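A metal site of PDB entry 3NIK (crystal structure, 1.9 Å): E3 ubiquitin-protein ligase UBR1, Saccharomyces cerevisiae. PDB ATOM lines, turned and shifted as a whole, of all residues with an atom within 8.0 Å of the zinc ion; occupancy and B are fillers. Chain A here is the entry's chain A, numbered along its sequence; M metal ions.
The backbone NH of Glu 26 sits close to the side-chain sulfur of Cys 24 (3.5 Å).
The zinc ion is bound by a ring nitrogen (ND1) of His 45, a ring nitrogen (ND1) of His 48, the side-chain sulfur of Cys 24 and the side-chain sulfur of Cys 27. The zinc ion has four donor atoms within binding distance.
Merely in contact with the zinc ion: Asp 44 (3.9 Å). Within 4 Å of the zinc ion: Cys 24, Cys 27, Asp 44, His 45 and His 48.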
ATOM      1  N   ARG A  23       0.278 -10.175  27.483  1.00  0.00           N
ATOM      2  CA  ARG A  23       0.373 -10.339  26.056  1.00  0.00           C
ATOM      3  C   ARG A  23      -1.063 -10.428  25.556  1.00  0.00           C
ATOM      4  O   ARG A  23      -1.872 -11.126  26.149  1.00  0.00           O
ATOM      5  CB  ARG A  23       1.119 -11.656  25.829  1.00  0.00           C
ATOM      6  CG  ARG A  23       1.532 -12.017  24.432  1.00  0.00           C
ATOM      7  CD  ARG A  23       2.780 -12.939  24.497  1.00  0.00           C
ATOM      8  NE  ARG A  23       3.976 -12.218  24.967  1.00  0.00           N
ATOM      9  CZ  ARG A  23       5.226 -12.699  24.916  1.00  0.00           C
ATOM     10  NH1 ARG A  23       5.469 -13.904  24.416  1.00  0.00           N
ATOM     11  NH2 ARG A  23       6.223 -11.964  25.367  1.00  0.00           N
ATOM     12  N   CYS A  24      -1.418  -9.683  24.514  1.00  0.00           N
ATOM     13  CA  CYS A  24      -2.731  -9.873  23.891  1.00  0.00           C
ATOM     14  C   CYS A  24      -2.599 -10.230  22.435  1.00  0.00           C
ATOM     15  O   CYS A  24      -2.028  -9.459  21.649  1.00  0.00           O
ATOM     16  CB  CYS A  24      -3.648  -8.666  24.070  1.00  0.00           C
ATOM     17  SG  CYS A  24      -5.218  -8.827  23.173  1.00  0.00           S
ATOM     18  N   HIS A  25      -3.128 -11.398  22.064  1.00  0.00           N
ATOM     19  CA  HIS A  25      -3.019 -11.845  20.687  1.00  0.00           C
ATOM     20  C   HIS A  25      -3.639 -10.843  19.724  1.00  0.00           C
ATOM     21  O   HIS A  25      -3.051 -10.532  18.697  1.00  0.00           O
ATOM     22  CB  HIS A  25      -3.636 -13.233  20.484  1.00  0.00           C
ATOM     23  CG  HIS A  25      -3.541 -13.717  19.075  1.00  0.00           C
ATOM     24  ND1 HIS A  25      -4.553 -13.531  18.151  1.00  0.00           N
ATOM     25  CD2 HIS A  25      -2.524 -14.319  18.411  1.00  0.00           C
ATOM     26  CE1 HIS A  25      -4.180 -14.029  16.990  1.00  0.00           C
ATOM     27  NE2 HIS A  25      -2.955 -14.512  17.125  1.00  0.00           N
ATOM     28  N   GLU A  26      -4.817 -10.334  20.084  1.00  0.00           N
ATOM     29  CA  GLU A  26      -5.579  -9.439  19.225  1.00  0.00           C
ATOM     30  C   GLU A  26      -5.027  -8.020  19.144  1.00  0.00           C
ATOM     31  O   GLU A  26      -5.106  -7.378  18.086  1.00  0.00           O
ATOM     32  CB  GLU A  26      -7.038  -9.391  19.684  1.00  0.00           C
ATOM     33  CG  GLU A  26      -7.864 -10.639  19.331  1.00  0.00           C
ATOM     34  CD  GLU A  26      -7.715 -11.785  20.319  1.00  0.00           C
ATOM     35  OE1 GLU A  26      -6.854 -11.712  21.229  1.00  0.00           O
ATOM     36  OE2 GLU A  26      -8.460 -12.799  20.188  1.00  0.00           O
ATOM     37  N   CYS A  27      -4.494  -7.506  20.249  1.00  0.00           N
ATOM     38  CA  CYS A  27      -4.043  -6.112  20.296  1.00  0.00           C
ATOM     39  C   CYS A  27      -2.588  -5.886  19.915  1.00  0.00           C
ATOM     40  O   CYS A  27      -2.250  -4.842  19.354  1.00  0.00           O
ATOM     41  CB  CYS A  27      -4.337  -5.515  21.669  1.00  0.00           C
ATOM     42  SG  CYS A  27      -6.098  -5.276  21.965  1.00  0.00           S
ATOM     43  N   GLY A  28      -1.728  -6.835  20.245  1.00  0.00           N
ATOM     44  CA  GLY A  28      -0.290  -6.691  20.058  1.00  0.00           C
ATOM     45  C   GLY A  28       0.125  -6.743  18.601  1.00  0.00           C
ATOM     46  O   GLY A  28      -0.369  -7.570  17.837  1.00  0.00           O
ATOM     47  N   LEU A  35       2.480  -5.608  28.296  1.00  0.00           N
ATOM     48  CA  LEU A  35       1.940  -4.586  29.185  1.00  0.00           C
ATOM     49  C   LEU A  35       2.198  -4.957  30.624  1.00  0.00           C
ATOM     50  O   LEU A  35       2.142  -6.139  30.990  1.00  0.00           O
ATOM     51  CB  LEU A  35       0.425  -4.422  28.966  1.00  0.00           C
ATOM     52  CG  LEU A  35       0.005  -3.908  27.591  1.00  0.00           C
ATOM     53  CD1 LEU A  35      -1.506  -4.093  27.346  1.00  0.00           C
ATOM     54  CD2 LEU A  35       0.388  -2.437  27.411  1.00  0.00           C
ATOM     55  N   PHE A  40      -2.060  -2.604  32.081  1.00  0.00           N
ATOM     56  CA  PHE A  40      -2.971  -3.573  31.469  1.00  0.00           C
ATOM     57  C   PHE A  40      -4.380  -3.332  31.969  1.00  0.00           C
ATOM     58  O   PHE A  40      -4.619  -3.381  33.172  1.00  0.00           O
ATOM     59  CB  PHE A  40      -2.529  -4.991  31.816  1.00  0.00           C
ATOM     60  CG  PHE A  40      -3.471  -6.063  31.314  1.00  0.00           C
ATOM     61  CD1 PHE A  40      -3.422  -6.477  29.991  1.00  0.00           C
ATOM     62  CD2 PHE A  40      -4.415  -6.644  32.168  1.00  0.00           C
ATOM     63  CE1 PHE A  40      -4.280  -7.468  29.521  1.00  0.00           C
ATOM     64  CE2 PHE A  40      -5.291  -7.643  31.708  1.00  0.00           C
ATOM     65  CZ  PHE A  40      -5.232  -8.050  30.397  1.00  0.00           C
ATOM     66  N   ASN A  41      -5.296  -3.058  31.038  1.00  0.00           N
ATOM     67  CA  ASN A  41      -6.679  -2.762  31.395  1.00  0.00           C
ATOM     68  C   ASN A  41      -7.561  -3.919  30.927  1.00  0.00           C
ATOM     69  O   ASN A  41      -7.806  -4.063  29.740  1.00  0.00           O
ATOM     70  CB  ASN A  41      -7.137  -1.440  30.758  1.00  0.00           C
ATOM     71  CG  ASN A  41      -8.522  -0.993  31.240  1.00  0.00           C
ATOM     72  OD1 ASN A  41      -9.313  -1.789  31.753  1.00  0.00           O
ATOM     73  ND2 ASN A  41      -8.803   0.303  31.089  1.00  0.00           N
ATOM     74  N   PRO A  42      -8.026  -4.750  31.867  1.00  0.00           N
ATOM     75  CA  PRO A  42      -8.790  -5.937  31.486  1.00  0.00           C
ATOM     76  C   PRO A  42      -9.979  -5.623  30.563  1.00  0.00           C
ATOM     77  O   PRO A  42     -10.333  -6.467  29.730  1.00  0.00           O
ATOM     78  CB  PRO A  42      -9.267  -6.500  32.816  1.00  0.00           C
ATOM     79  CG  PRO A  42      -8.220  -6.029  33.799  1.00  0.00           C
ATOM     80  CD  PRO A  42      -7.893  -4.643  33.330  1.00  0.00           C
ATOM     81  N   LYS A  43     -10.542  -4.422  30.679  1.00  0.00           N
ATOM     82  CA  LYS A  43     -11.685  -4.002  29.846  1.00  0.00           C
ATOM     83  C   LYS A  43     -11.338  -3.888  28.346  1.00  0.00           C
ATOM     84  O   LYS A  43     -12.214  -4.097  27.487  1.00  0.00           O
ATOM     85  CB  LYS A  43     -12.275  -2.680  30.345  1.00  0.00           C
ATOM     86  CG  LYS A  43     -12.948  -2.762  31.706  1.00  0.00           C
ATOM     87  CD  LYS A  43     -13.674  -1.459  32.082  1.00  0.00           C
ATOM     88  CE  LYS A  43     -12.710  -0.355  32.506  1.00  0.00           C
ATOM     89  NZ  LYS A  43     -13.413   0.916  32.914  1.00  0.00           N
ATOM     90  N   ASP A  44     -10.090  -3.555  28.047  1.00  0.00           N
ATOM     91  CA  ASP A  44      -9.622  -3.500  26.655  1.00  0.00           C
ATOM     92  C   ASP A  44      -9.609  -4.882  25.997  1.00  0.00           C
ATOM     93  O   ASP A  44      -9.608  -4.970  24.773  1.00  0.00           O
ATOM     94  CB  ASP A  44      -8.198  -2.921  26.558  1.00  0.00           C
ATOM     95  CG  ASP A  44      -8.122  -1.430  26.827  1.00  0.00           C
ATOM     96  OD1 ASP A  44      -9.121  -0.678  26.654  1.00  0.00           O
ATOM     97  OD2 ASP A  44      -7.005  -0.994  27.177  1.00  0.00           O
ATOM     98  N   HIS A  45      -9.588  -5.935  26.812  1.00  0.00           N
ATOM     99  CA  HIS A  45      -9.255  -7.285  26.349  1.00  0.00           C
ATOM    100  C   HIS A  45     -10.272  -8.356  26.749  1.00  0.00           C
ATOM    101  O   HIS A  45      -9.946  -9.547  26.795  1.00  0.00           O
ATOM    102  CB  HIS A  45      -7.853  -7.667  26.828  1.00  0.00           C
ATOM    103  CG  HIS A  45      -6.840  -6.578  26.608  1.00  0.00           C
ATOM    104  ND1 HIS A  45      -6.264  -6.345  25.384  1.00  0.00           N
ATOM    105  CD2 HIS A  45      -6.365  -5.625  27.443  1.00  0.00           C
ATOM    106  CE1 HIS A  45      -5.448  -5.298  25.471  1.00  0.00           C
ATOM    107  NE2 HIS A  45      -5.482  -4.859  26.719  1.00  0.00           N
ATOM    108  N   VAL A  46     -11.501  -7.918  27.021  1.00  0.00           N
ATOM    109  CA  VAL A  46     -12.613  -8.804  27.405  1.00  0.00           C
ATOM    110  C   VAL A  46     -12.836  -9.969  26.426  1.00  0.00           C
ATOM    111  O   VAL A  46     -13.020 -11.121  26.844  1.00  0.00           O
ATOM    112  CB  VAL A  46     -13.923  -7.987  27.543  1.00  0.00           C
ATOM    113  CG1 VAL A  46     -15.170  -8.904  27.630  1.00  0.00           C
ATOM    114  CG2 VAL A  46     -13.841  -7.061  28.745  1.00  0.00           C
ATOM    115  N   ASN A  47     -12.822  -9.660  25.137  1.00  0.00           N
ATOM    116  CA  ASN A  47     -13.066 -10.653  24.106  1.00  0.00           C
ATOM    117  C   ASN A  47     -11.779 -11.172  23.501  1.00  0.00           C
ATOM    118  O   ASN A  47     -11.780 -11.732  22.401  1.00  0.00           O
ATOM    119  CB  ASN A  47     -13.944 -10.048  22.998  1.00  0.00           C
ATOM    120  CG  ASN A  47     -15.164  -9.316  23.547  1.00  0.00           C
ATOM    121  OD1 ASN A  47     -15.947  -9.882  24.317  1.00  0.00           O
ATOM    122  ND2 ASN A  47     -15.329  -8.059  23.135  1.00  0.00           N
ATOM    123  N   HIS A  48     -10.668 -10.997  24.214  1.00  0.00           N
ATOM    124  CA  HIS A  48      -9.365 -11.275  23.642  1.00  0.00           C
ATOM    125  C   HIS A  48      -8.618 -12.442  24.296  1.00  0.00           C
ATOM    126  O   HIS A  48      -8.876 -12.791  25.454  1.00  0.00           O
ATOM    127  CB  HIS A  48      -8.504 -10.002  23.641  1.00  0.00           C
ATOM    128  CG  HIS A  48      -9.032  -8.918  22.752  1.00  0.00           C
ATOM    129  ND1 HIS A  48      -8.515  -7.638  22.739  1.00  0.00           N
ATOM    130  CD2 HIS A  48     -10.037  -8.928  21.840  1.00  0.00           C
ATOM    131  CE1 HIS A  48      -9.168  -6.908  21.850  1.00  0.00           C
ATOM    132  NE2 HIS A  48     -10.102  -7.659  21.307  1.00  0.00           N
ATOM    133  N   HIS A  49      -7.699 -13.023  23.535  1.00  0.00           N
ATOM    134  CA  HIS A  49      -6.823 -14.086  24.016  1.00  0.00           C
ATOM    135  C   HIS A  49      -5.587 -13.435  24.617  1.00  0.00           C
ATOM    136  O   HIS A  49      -4.718 -12.933  23.904  1.00  0.00           O
ATOM    137  CB  HIS A  49      -6.437 -15.019  22.881  1.00  0.00           C
ATOM    138  CG  HIS A  49      -7.608 -15.715  22.261  1.00  0.00           C
ATOM    139  ND1 HIS A  49      -8.442 -15.108  21.353  1.00  0.00           N
ATOM    140  CD2 HIS A  49      -8.077 -16.982  22.415  1.00  0.00           C
ATOM    141  CE1 HIS A  49      -9.379 -15.963  20.974  1.00  0.00           C
ATOM    142  NE2 HIS A  49      -9.178 -17.104  21.605  1.00  0.00           N
ATOM    143  N   VAL A  50      -5.568 -13.431  25.947  1.00  0.00           N
ATOM    144  CA  VAL A  50      -4.520 -12.798  26.752  1.00  0.00           C
ATOM    145  C   VAL A  50      -3.744 -13.867  27.506  1.00  0.00           C
ATOM    146  O   VAL A  50      -4.318 -14.843  27.981  1.00  0.00           O
ATOM    147  CB  VAL A  50      -5.138 -11.809  27.772  1.00  0.00           C
ATOM    148  CG1 VAL A  50      -4.086 -11.261  28.730  1.00  0.00           C
ATOM    149  CG2 VAL A  50      -5.842 -10.689  27.054  1.00  0.00           C
ATOM    150  N   TRP A  71       0.868  -1.610  19.027  1.00  0.00           N
ATOM    151  CA  TRP A  71      -0.540  -1.953  19.251  1.00  0.00           C
ATOM    152  C   TRP A  71      -1.443  -1.695  18.065  1.00  0.00           C
ATOM    153  O   TRP A  71      -1.398  -0.603  17.459  1.00  0.00           O
ATOM    154  CB  TRP A  71      -1.096  -1.240  20.505  1.00  0.00           C
ATOM    155  CG  TRP A  71      -0.242  -1.521  21.687  1.00  0.00           C
ATOM    156  CD1 TRP A  71       0.666  -0.675  22.268  1.00  0.00           C
ATOM    157  CD2 TRP A  71      -0.150  -2.763  22.394  1.00  0.00           C
ATOM    158  NE1 TRP A  71       1.312  -1.306  23.292  1.00  0.00           N
ATOM    159  CE2 TRP A  71       0.831  -2.587  23.399  1.00  0.00           C
ATOM    160  CE3 TRP A  71      -0.793  -3.997  22.292  1.00  0.00           C
ATOM    161  CZ2 TRP A  71       1.172  -3.602  24.301  1.00  0.00           C
ATOM    162  CZ3 TRP A  71      -0.455  -5.013  23.181  1.00  0.00           C
ATOM    163  CH2 TRP A  71       0.529  -4.813  24.171  1.00  0.00           C
ATOM    164  N   SER A  73      -4.817  -1.759  18.284  1.00  0.00           N
ATOM    165  CA  SER A  73      -6.040  -1.092  18.735  1.00  0.00           C
ATOM    166  C   SER A  73      -5.713  -0.070  19.820  1.00  0.00           C
ATOM    167  O   SER A  73      -4.677  -0.185  20.471  1.00  0.00           O
ATOM    168  CB  SER A  73      -7.050  -2.126  19.255  1.00  0.00           C
ATOM    169  OG  SER A  73      -7.426  -3.061  18.255  1.00  0.00           O
ATOM    170  N   PRO A  74      -6.591   0.921  20.012  1.00  0.00           N
ATOM    171  CA  PRO A  74      -6.285   1.899  21.068  1.00  0.00           C
ATOM    172  C   PRO A  74      -6.328   1.243  22.445  1.00  0.00           C
ATOM    173  O   PRO A  74      -7.264   0.491  22.747  1.00  0.00           O
ATOM    174  CB  PRO A  74      -7.398   2.945  20.936  1.00  0.00           C
ATOM    175  CG  PRO A  74      -8.479   2.290  20.146  1.00  0.00           C
ATOM    176  CD  PRO A  74      -7.842   1.234  19.297  1.00  0.00           C
ATOM    177  N   LEU A  75      -5.301   1.489  23.266  1.00  0.00           N
ATOM    178  CA  LEU A  75      -5.314   1.023  24.653  1.00  0.00           C
ATOM    179  C   LEU A  75      -5.779   2.114  25.604  1.00  0.00           C
ATOM    180  O   LEU A  75      -5.555   3.296  25.364  1.00  0.00           O
ATOM    181  CB  LEU A  75      -3.926   0.546  25.102  1.00  0.00           C
ATOM    182  CG  LEU A  75      -3.237  -0.601  24.353  1.00  0.00           C
ATOM    183  CD1 LEU A  75      -1.880  -0.860  24.960  1.00  0.00           C
ATOM    184  CD2 LEU A  75      -4.064  -1.876  24.369  1.00  0.00           C
HETATM  185 ZN    ZN M   1      -6.548  -7.069  23.458  1.00  0.00          ZN
